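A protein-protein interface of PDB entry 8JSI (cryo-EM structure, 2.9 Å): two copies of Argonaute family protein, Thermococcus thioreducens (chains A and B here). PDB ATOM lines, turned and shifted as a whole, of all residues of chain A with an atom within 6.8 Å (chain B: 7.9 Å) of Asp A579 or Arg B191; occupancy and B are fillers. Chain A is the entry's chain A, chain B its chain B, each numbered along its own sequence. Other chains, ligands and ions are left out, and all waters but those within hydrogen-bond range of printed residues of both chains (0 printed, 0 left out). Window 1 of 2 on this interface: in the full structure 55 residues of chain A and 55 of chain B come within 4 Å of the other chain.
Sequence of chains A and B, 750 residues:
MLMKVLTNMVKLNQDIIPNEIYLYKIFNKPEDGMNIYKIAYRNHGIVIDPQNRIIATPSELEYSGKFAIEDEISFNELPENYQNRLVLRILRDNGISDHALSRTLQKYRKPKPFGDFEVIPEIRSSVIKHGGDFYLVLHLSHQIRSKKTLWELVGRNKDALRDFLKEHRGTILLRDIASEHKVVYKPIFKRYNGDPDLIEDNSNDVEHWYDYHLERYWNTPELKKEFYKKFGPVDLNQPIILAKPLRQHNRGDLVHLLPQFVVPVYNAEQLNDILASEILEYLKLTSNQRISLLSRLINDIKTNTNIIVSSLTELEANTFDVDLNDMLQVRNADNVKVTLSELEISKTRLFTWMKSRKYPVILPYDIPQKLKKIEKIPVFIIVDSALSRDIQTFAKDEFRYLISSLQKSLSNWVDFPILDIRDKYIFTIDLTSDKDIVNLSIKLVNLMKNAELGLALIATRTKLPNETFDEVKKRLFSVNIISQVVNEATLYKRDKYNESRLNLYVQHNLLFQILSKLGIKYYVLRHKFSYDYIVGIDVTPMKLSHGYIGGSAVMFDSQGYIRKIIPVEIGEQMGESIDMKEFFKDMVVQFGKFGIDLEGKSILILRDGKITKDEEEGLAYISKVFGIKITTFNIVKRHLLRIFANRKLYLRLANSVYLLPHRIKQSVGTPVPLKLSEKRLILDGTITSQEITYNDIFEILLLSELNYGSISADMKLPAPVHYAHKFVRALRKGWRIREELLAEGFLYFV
Among the printed residues, Asp or Glu carboxylates within 4 Å of a Lys or Arg side-chain nitrogen of the other chain: Asp A579 with Arg B191 (3.97 Å), Lys A581 with Asp B434 (3.2 Å) and Asp A614 with Arg B191 (2.8 Å).
Lys A581 touches Tyr B192. CA of Gly A618 touches OH of Tyr B192 (3.4 Å).
No position is printed for both chains. Of the 5 pairs that touch across the chains among the printed residues, none has its exchanged pair printed and touching as well.
The side-chain carboxylate (OD1) of Asp A579 is in salt-bridge range of the guanidinium group (NH1) of Arg B191. The side-chain carboxylate (OD2) of Asp B434 is in salt-bridge range of the side-chain amino group (NZ) of Lys A581 (3.2 Å). The side-chain carboxylate (OD2) of Asp A614 is in salt-bridge range of the guanidinium group (NH2) of Arg B191 (2.8 Å).
Of chain B, only Arg B191 comes within 4 Å of Asp A579. Met A580 touches none of the printed residues of chain B. Of the printed residues of chain B, Lys A581 touches Tyr B192 and Asp B434. Of the printed residues of chain A, Arg B191 touches Asp A579 (3.97 Å) and Asp A614 (2.8 Å). Of the printed residues of chain A, Tyr B192 touches Lys A581 (3.6 Å) and Gly A618 (3.4 Å). Of the printed residues of chain A, Asp B434 touches Lys A581 (3.2 Å). The nearest printed residue of chain B that does not touch Gly A618 is Arg B191 (6.8 Å).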
ATOM      1  N   ILE A 570       4.473 -32.581  -7.538  1.00  0.00           N
ATOM      2  CA  ILE A 570       4.867 -31.233  -7.938  1.00  0.00           C
ATOM      3  C   ILE A 570       5.945 -31.288  -9.009  1.00  0.00           C
ATOM      4  O   ILE A 570       5.801 -30.720 -10.097  1.00  0.00           O
ATOM      5  CB  ILE A 570       5.340 -30.418  -6.721  1.00  0.00           C
ATOM      6  CG1 ILE A 570       4.254 -30.356  -5.649  1.00  0.00           C
ATOM      7  CG2 ILE A 570       5.758 -29.024  -7.149  1.00  0.00           C
ATOM      8  CD1 ILE A 570       2.896 -30.040  -6.186  1.00  0.00           C
ATOM      9  N   GLN A 573      12.948 -30.166  -7.348  1.00  0.00           N
ATOM     10  CA  GLN A 573      13.506 -28.883  -6.950  1.00  0.00           C
ATOM     11  C   GLN A 573      14.941 -29.062  -6.483  1.00  0.00           C
ATOM     12  O   GLN A 573      15.424 -30.180  -6.281  1.00  0.00           O
ATOM     13  CB  GLN A 573      12.675 -28.232  -5.837  1.00  0.00           C
ATOM     14  CG  GLN A 573      11.189 -28.489  -5.937  1.00  0.00           C
ATOM     15  CD  GLN A 573      10.532 -28.579  -4.580  1.00  0.00           C
ATOM     16  OE1 GLN A 573      11.091 -28.138  -3.579  1.00  0.00           O
ATOM     17  NE2 GLN A 573       9.342 -29.157  -4.539  1.00  0.00           N
ATOM     18  N   SER A 577      11.521 -25.095  -2.018  1.00  0.00           N
ATOM     19  CA  SER A 577      10.731 -23.980  -2.535  1.00  0.00           C
ATOM     20  C   SER A 577       9.877 -24.519  -3.683  1.00  0.00           C
ATOM     21  O   SER A 577      10.387 -24.728  -4.786  1.00  0.00           O
ATOM     22  CB  SER A 577      11.621 -22.836  -2.991  1.00  0.00           C
ATOM     23  OG  SER A 577      10.948 -22.006  -3.918  1.00  0.00           O
ATOM     24  N   ILE A 578       8.590 -24.738  -3.410  1.00  0.00           N
ATOM     25  CA  ILE A 578       7.685 -25.255  -4.427  1.00  0.00           C
ATOM     26  C   ILE A 578       7.529 -24.238  -5.551  1.00  0.00           C
ATOM     27  O   ILE A 578       7.428 -23.026  -5.319  1.00  0.00           O
ATOM     28  CB  ILE A 578       6.321 -25.606  -3.806  1.00  0.00           C
ATOM     29  CG1 ILE A 578       6.496 -26.528  -2.599  1.00  0.00           C
ATOM     30  CG2 ILE A 578       5.408 -26.245  -4.839  1.00  0.00           C
ATOM     31  CD1 ILE A 578       6.702 -27.976  -2.961  1.00  0.00           C
ATOM     32  N   ASP A 579       7.520 -24.733  -6.787  1.00  0.00           N
ATOM     33  CA  ASP A 579       7.235 -23.906  -7.957  1.00  0.00           C
ATOM     34  C   ASP A 579       5.727 -23.911  -8.170  1.00  0.00           C
ATOM     35  O   ASP A 579       5.180 -24.818  -8.799  1.00  0.00           O
ATOM     36  CB  ASP A 579       7.975 -24.423  -9.184  1.00  0.00           C
ATOM     37  CG  ASP A 579       8.312 -23.321 -10.165  1.00  0.00           C
ATOM     38  OD1 ASP A 579       9.294 -22.589  -9.924  1.00  0.00           O
ATOM     39  OD2 ASP A 579       7.595 -23.187 -11.179  1.00  0.00           O
ATOM     40  N   MET A 580       5.049 -22.892  -7.640  1.00  0.00           N
ATOM     41  CA  MET A 580       3.592 -22.870  -7.689  1.00  0.00           C
ATOM     42  C   MET A 580       3.053 -22.553  -9.076  1.00  0.00           C
ATOM     43  O   MET A 580       1.880 -22.820  -9.347  1.00  0.00           O
ATOM     44  CB  MET A 580       3.045 -21.869  -6.673  1.00  0.00           C
ATOM     45  CG  MET A 580       3.444 -22.172  -5.244  1.00  0.00           C
ATOM     46  SD  MET A 580       2.333 -23.380  -4.502  1.00  0.00           S
ATOM     47  CE  MET A 580       3.033 -23.527  -2.864  1.00  0.00           C
ATOM     48  N   LYS A 581       3.877 -22.005  -9.969  1.00  0.00           N
ATOM     49  CA  LYS A 581       3.392 -21.692 -11.310  1.00  0.00           C
ATOM     50  C   LYS A 581       3.153 -22.966 -12.116  1.00  0.00           C
ATOM     51  O   LYS A 581       2.043 -23.205 -12.609  1.00  0.00           O
ATOM     52  CB  LYS A 581       4.383 -20.771 -12.021  1.00  0.00           C
ATOM     53  CG  LYS A 581       3.734 -19.817 -13.005  1.00  0.00           C
ATOM     54  CD  LYS A 581       4.733 -19.318 -14.032  1.00  0.00           C
ATOM     55  CE  LYS A 581       4.447 -19.887 -15.408  1.00  0.00           C
ATOM     56  NZ  LYS A 581       5.459 -19.449 -16.408  1.00  0.00           N
ATOM     57  N   GLU A 582       4.187 -23.799 -12.261  1.00  0.00           N
ATOM     58  CA  GLU A 582       4.022 -25.076 -12.949  1.00  0.00           C
ATOM     59  C   GLU A 582       3.050 -25.979 -12.200  1.00  0.00           C
ATOM     60  O   GLU A 582       2.229 -26.673 -12.819  1.00  0.00           O
ATOM     61  CB  GLU A 582       5.374 -25.769 -13.104  1.00  0.00           C
ATOM     62  CG  GLU A 582       6.319 -25.105 -14.090  1.00  0.00           C
ATOM     63  CD  GLU A 582       5.684 -24.875 -15.446  1.00  0.00           C
ATOM     64  OE1 GLU A 582       5.240 -25.859 -16.074  1.00  0.00           O
ATOM     65  OE2 GLU A 582       5.644 -23.710 -15.892  1.00  0.00           O
ATOM     66  N   PHE A 583       3.147 -25.991 -10.867  1.00  0.00           N
ATOM     67  CA  PHE A 583       2.221 -26.775 -10.059  1.00  0.00           C
ATOM     68  C   PHE A 583       0.783 -26.388 -10.366  1.00  0.00           C
ATOM     69  O   PHE A 583      -0.059 -27.258 -10.591  1.00  0.00           O
ATOM     70  CB  PHE A 583       2.532 -26.583  -8.571  1.00  0.00           C
ATOM     71  CG  PHE A 583       1.427 -27.030  -7.636  1.00  0.00           C
ATOM     72  CD1 PHE A 583       0.676 -28.169  -7.891  1.00  0.00           C
ATOM     73  CD2 PHE A 583       1.188 -26.338  -6.461  1.00  0.00           C
ATOM     74  CE1 PHE A 583      -0.321 -28.570  -7.028  1.00  0.00           C
ATOM     75  CE2 PHE A 583       0.190 -26.735  -5.594  1.00  0.00           C
ATOM     76  CZ  PHE A 583      -0.562 -27.854  -5.878  1.00  0.00           C
ATOM     77  N   PHE A 584       0.486 -25.091 -10.413  1.00  0.00           N
ATOM     78  CA  PHE A 584      -0.893 -24.678 -10.629  1.00  0.00           C
ATOM     79  C   PHE A 584      -1.322 -24.825 -12.081  1.00  0.00           C
ATOM     80  O   PHE A 584      -2.514 -25.006 -12.352  1.00  0.00           O
ATOM     81  CB  PHE A 584      -1.098 -23.247 -10.140  1.00  0.00           C
ATOM     82  CG  PHE A 584      -1.854 -23.167  -8.851  1.00  0.00           C
ATOM     83  CD1 PHE A 584      -3.225 -23.350  -8.829  1.00  0.00           C
ATOM     84  CD2 PHE A 584      -1.194 -22.947  -7.658  1.00  0.00           C
ATOM     85  CE1 PHE A 584      -3.925 -23.292  -7.644  1.00  0.00           C
ATOM     86  CE2 PHE A 584      -1.888 -22.890  -6.471  1.00  0.00           C
ATOM     87  CZ  PHE A 584      -3.255 -23.062  -6.463  1.00  0.00           C
ATOM     88  N   LYS A 613       9.006 -16.693  -0.216  1.00  0.00           N
ATOM     89  CA  LYS A 613       8.691 -15.541  -1.058  1.00  0.00           C
ATOM     90  C   LYS A 613       8.397 -15.965  -2.492  1.00  0.00           C
ATOM     91  O   LYS A 613       7.497 -15.415  -3.140  1.00  0.00           O
ATOM     92  CB  LYS A 613       9.844 -14.537  -1.027  1.00  0.00           C
ATOM     93  CG  LYS A 613       9.670 -13.401  -0.033  1.00  0.00           C
ATOM     94  CD  LYS A 613       9.722 -13.897   1.401  1.00  0.00           C
ATOM     95  CE  LYS A 613       9.676 -12.740   2.388  1.00  0.00           C
ATOM     96  NZ  LYS A 613       8.484 -11.872   2.182  1.00  0.00           N
ATOM     97  N   ASP A 614       9.155 -16.933  -3.009  1.00  0.00           N
ATOM     98  CA  ASP A 614       8.945 -17.389  -4.378  1.00  0.00           C
ATOM     99  C   ASP A 614       7.570 -18.024  -4.545  1.00  0.00           C
ATOM    100  O   ASP A 614       6.893 -17.795  -5.556  1.00  0.00           O
ATOM    101  CB  ASP A 614      10.047 -18.368  -4.776  1.00  0.00           C
ATOM    102  CG  ASP A 614      11.430 -17.846  -4.443  1.00  0.00           C
ATOM    103  OD1 ASP A 614      11.692 -17.572  -3.254  1.00  0.00           O
ATOM    104  OD2 ASP A 614      12.256 -17.709  -5.369  1.00  0.00           O
ATOM    105  N   GLU A 615       7.138 -18.823  -3.567  1.00  0.00           N
ATOM    106  CA  GLU A 615       5.787 -19.367  -3.607  1.00  0.00           C
ATOM    107  C   GLU A 615       4.740 -18.265  -3.529  1.00  0.00           C
ATOM    108  O   GLU A 615       3.696 -18.359  -4.185  1.00  0.00           O
ATOM    109  CB  GLU A 615       5.590 -20.374  -2.476  1.00  0.00           C
ATOM    110  CG  GLU A 615       6.564 -21.537  -2.508  1.00  0.00           C
ATOM    111  CD  GLU A 615       6.277 -22.569  -1.436  1.00  0.00           C
ATOM    112  OE1 GLU A 615       5.219 -22.471  -0.782  1.00  0.00           O
ATOM    113  OE2 GLU A 615       7.110 -23.479  -1.246  1.00  0.00           O
ATOM    114  N   GLU A 617       5.051 -15.181  -4.742  1.00  0.00           N
ATOM    115  CA  GLU A 617       4.987 -14.558  -6.060  1.00  0.00           C
ATOM    116  C   GLU A 617       4.299 -15.468  -7.071  1.00  0.00           C
ATOM    117  O   GLU A 617       3.515 -14.996  -7.904  1.00  0.00           O
ATOM    118  CB  GLU A 617       6.390 -14.188  -6.535  1.00  0.00           C
ATOM    119  CG  GLU A 617       7.127 -13.248  -5.599  1.00  0.00           C
ATOM    120  CD  GLU A 617       8.514 -12.897  -6.099  1.00  0.00           C
ATOM    121  OE1 GLU A 617       8.799 -13.150  -7.288  1.00  0.00           O
ATOM    122  OE2 GLU A 617       9.318 -12.368  -5.304  1.00  0.00           O
ATOM    123  N   GLY A 618       4.578 -16.772  -7.013  1.00  0.00           N
ATOM    124  CA  GLY A 618       3.912 -17.697  -7.915  1.00  0.00           C
ATOM    125  C   GLY A 618       2.411 -17.738  -7.708  1.00  0.00           C
ATOM    126  O   GLY A 618       1.641 -17.731  -8.672  1.00  0.00           O
ATOM    127  N   ILE B 188      20.472 -11.884 -13.066  1.00  0.00           N
ATOM    128  CA  ILE B 188      19.157 -12.257 -12.557  1.00  0.00           C
ATOM    129  C   ILE B 188      18.110 -11.423 -13.279  1.00  0.00           C
ATOM    130  O   ILE B 188      18.245 -10.197 -13.380  1.00  0.00           O
ATOM    131  CB  ILE B 188      19.067 -12.065 -11.033  1.00  0.00           C
ATOM    132  CG1 ILE B 188      19.521 -13.333 -10.313  1.00  0.00           C
ATOM    133  CG2 ILE B 188      17.653 -11.708 -10.612  1.00  0.00           C
ATOM    134  CD1 ILE B 188      19.936 -13.098  -8.885  1.00  0.00           C
ATOM    135  N   PHE B 189      17.075 -12.087 -13.786  1.00  0.00           N
ATOM    136  CA  PHE B 189      15.981 -11.437 -14.490  1.00  0.00           C
ATOM    137  C   PHE B 189      14.684 -11.645 -13.722  1.00  0.00           C
ATOM    138  O   PHE B 189      14.532 -12.625 -12.986  1.00  0.00           O
ATOM    139  CB  PHE B 189      15.835 -11.980 -15.916  1.00  0.00           C
ATOM    140  CG  PHE B 189      17.056 -11.785 -16.767  1.00  0.00           C
ATOM    141  CD1 PHE B 189      18.091 -12.704 -16.737  1.00  0.00           C
ATOM    142  CD2 PHE B 189      17.169 -10.686 -17.598  1.00  0.00           C
ATOM    143  CE1 PHE B 189      19.215 -12.526 -17.516  1.00  0.00           C
ATOM    144  CE2 PHE B 189      18.290 -10.504 -18.379  1.00  0.00           C
ATOM    145  CZ  PHE B 189      19.313 -11.425 -18.338  1.00  0.00           C
ATOM    146  N   LYS B 190      13.753 -10.711 -13.893  1.00  0.00           N
ATOM    147  CA  LYS B 190      12.442 -10.844 -13.269  1.00  0.00           C
ATOM    148  C   LYS B 190      11.731 -12.074 -13.816  1.00  0.00           C
ATOM    149  O   LYS B 190      11.736 -12.326 -15.024  1.00  0.00           O
ATOM    150  CB  LYS B 190      11.607  -9.589 -13.512  1.00  0.00           C
ATOM    151  CG  LYS B 190      12.391  -8.294 -13.389  1.00  0.00           C
ATOM    152  CD  LYS B 190      12.846  -8.053 -11.959  1.00  0.00           C
ATOM    153  CE  LYS B 190      12.366  -6.706 -11.445  1.00  0.00           C
ATOM    154  NZ  LYS B 190      12.777  -5.592 -12.345  1.00  0.00           N
ATOM    155  N   ARG B 191      11.116 -12.845 -12.917  1.00  0.00           N
ATOM    156  CA  ARG B 191      10.546 -14.132 -13.297  1.00  0.00           C
ATOM    157  C   ARG B 191       9.335 -13.998 -14.209  1.00  0.00           C
ATOM    158  O   ARG B 191       8.976 -14.970 -14.882  1.00  0.00           O
ATOM    159  CB  ARG B 191      10.164 -14.925 -12.047  1.00  0.00           C
ATOM    160  CG  ARG B 191      10.157 -16.429 -12.247  1.00  0.00           C
ATOM    161  CD  ARG B 191      11.376 -17.073 -11.610  1.00  0.00           C
ATOM    162  NE  ARG B 191      11.439 -16.810 -10.178  1.00  0.00           N
ATOM    163  CZ  ARG B 191      11.172 -17.707  -9.237  1.00  0.00           C
ATOM    164  NH1 ARG B 191      10.823 -18.945  -9.543  1.00  0.00           N
ATOM    165  NH2 ARG B 191      11.259 -17.351  -7.960  1.00  0.00           N
ATOM    166  N   TYR B 192       8.697 -12.831 -14.251  1.00  0.00           N
ATOM    167  CA  TYR B 192       7.478 -12.685 -15.036  1.00  0.00           C
ATOM    168  C   TYR B 192       7.554 -11.483 -15.968  1.00  0.00           C
ATOM    169  O   TYR B 192       6.970 -11.497 -17.056  1.00  0.00           O
ATOM    170  CB  TYR B 192       6.271 -12.576 -14.104  1.00  0.00           C
ATOM    171  CG  TYR B 192       6.156 -13.752 -13.161  1.00  0.00           C
ATOM    172  CD1 TYR B 192       5.938 -15.034 -13.646  1.00  0.00           C
ATOM    173  CD2 TYR B 192       6.287 -13.583 -11.790  1.00  0.00           C
ATOM    174  CE1 TYR B 192       5.841 -16.113 -12.793  1.00  0.00           C
ATOM    175  CE2 TYR B 192       6.191 -14.658 -10.928  1.00  0.00           C
ATOM    176  CZ  TYR B 192       5.969 -15.919 -11.435  1.00  0.00           C
ATOM    177  OH  TYR B 192       5.873 -16.993 -10.582  1.00  0.00           O
ATOM    178  N   ASN B 193       8.272 -10.439 -15.555  1.00  0.00           N
ATOM    179  CA  ASN B 193       8.451  -9.274 -16.409  1.00  0.00           C
ATOM    180  C   ASN B 193       9.458  -9.517 -17.525  1.00  0.00           C
ATOM    181  O   ASN B 193       9.406  -8.826 -18.549  1.00  0.00           O
ATOM    182  CB  ASN B 193       8.886  -8.069 -15.574  1.00  0.00           C
ATOM    183  CG  ASN B 193       8.815  -6.767 -16.347  1.00  0.00           C
ATOM    184  OD1 ASN B 193       8.013  -6.622 -17.270  1.00  0.00           O
ATOM    185  ND2 ASN B 193       9.657  -5.811 -15.976  1.00  0.00           N
ATOM    186  N   GLY B 194      10.358 -10.480 -17.358  1.00  0.00           N
ATOM    187  CA  GLY B 194      11.368 -10.743 -18.372  1.00  0.00           C
ATOM    188  C   GLY B 194      12.339  -9.599 -18.563  1.00  0.00           C
ATOM    189  O   GLY B 194      12.795  -9.353 -19.686  1.00  0.00           O
ATOM    190  N   ASP B 195      12.668  -8.892 -17.485  1.00  0.00           N
ATOM    191  CA  ASP B 195      13.553  -7.742 -17.524  1.00  0.00           C
ATOM    192  C   ASP B 195      14.748  -7.966 -16.606  1.00  0.00           C
ATOM    193  O   ASP B 195      14.639  -8.682 -15.606  1.00  0.00           O
ATOM    194  CB  ASP B 195      12.816  -6.467 -17.098  1.00  0.00           C
ATOM    195  CG  ASP B 195      13.085  -5.299 -18.022  1.00  0.00           C
ATOM    196  OD1 ASP B 195      13.372  -5.535 -19.213  1.00  0.00           O
ATOM    197  OD2 ASP B 195      13.011  -4.143 -17.558  1.00  0.00           O
ATOM    198  N   ASP B 197      17.369  -7.252 -13.637  1.00  0.00           N
ATOM    199  CA  ASP B 197      17.193  -6.679 -12.302  1.00  0.00           C
ATOM    200  C   ASP B 197      18.404  -5.805 -11.997  1.00  0.00           C
ATOM    201  O   ASP B 197      19.442  -6.284 -11.541  1.00  0.00           O
ATOM    202  CB  ASP B 197      17.012  -7.778 -11.263  1.00  0.00           C
ATOM    203  CG  ASP B 197      16.094  -7.365 -10.130  1.00  0.00           C
ATOM    204  OD1 ASP B 197      15.780  -6.162 -10.023  1.00  0.00           O
ATOM    205  OD2 ASP B 197      15.686  -8.247  -9.345  1.00  0.00           O
ATOM    206  N   ASP B 434       1.047 -18.498 -21.226  1.00  0.00           N
ATOM    207  CA  ASP B 434       0.770 -19.682 -20.422  1.00  0.00           C
ATOM    208  C   ASP B 434      -0.681 -20.135 -20.483  1.00  0.00           C
ATOM    209  O   ASP B 434      -0.940 -21.341 -20.447  1.00  0.00           O
ATOM    210  CB  ASP B 434       1.156 -19.430 -18.962  1.00  0.00           C
ATOM    211  CG  ASP B 434       2.655 -19.446 -18.747  1.00  0.00           C
ATOM    212  OD1 ASP B 434       3.261 -20.530 -18.871  1.00  0.00           O
ATOM    213  OD2 ASP B 434       3.227 -18.375 -18.458  1.00  0.00           O
ATOM    214  N   LEU B 544      19.019 -28.748 -12.951  1.00  0.00           N
ATOM    215  CA  LEU B 544      18.811 -27.965 -11.727  1.00  0.00           C
ATOM    216  C   LEU B 544      18.704 -28.873 -10.501  1.00  0.00           C
ATOM    217  O   LEU B 544      17.714 -28.863  -9.767  1.00  0.00           O
ATOM    218  CB  LEU B 544      17.557 -27.098 -11.838  1.00  0.00           C
ATOM    219  CG  LEU B 544      16.405 -27.503 -10.914  1.00  0.00           C
ATOM    220  CD1 LEU B 544      16.282 -26.544  -9.740  1.00  0.00           C
ATOM    221  CD2 LEU B 544      15.095 -27.591 -11.682  1.00  0.00           C
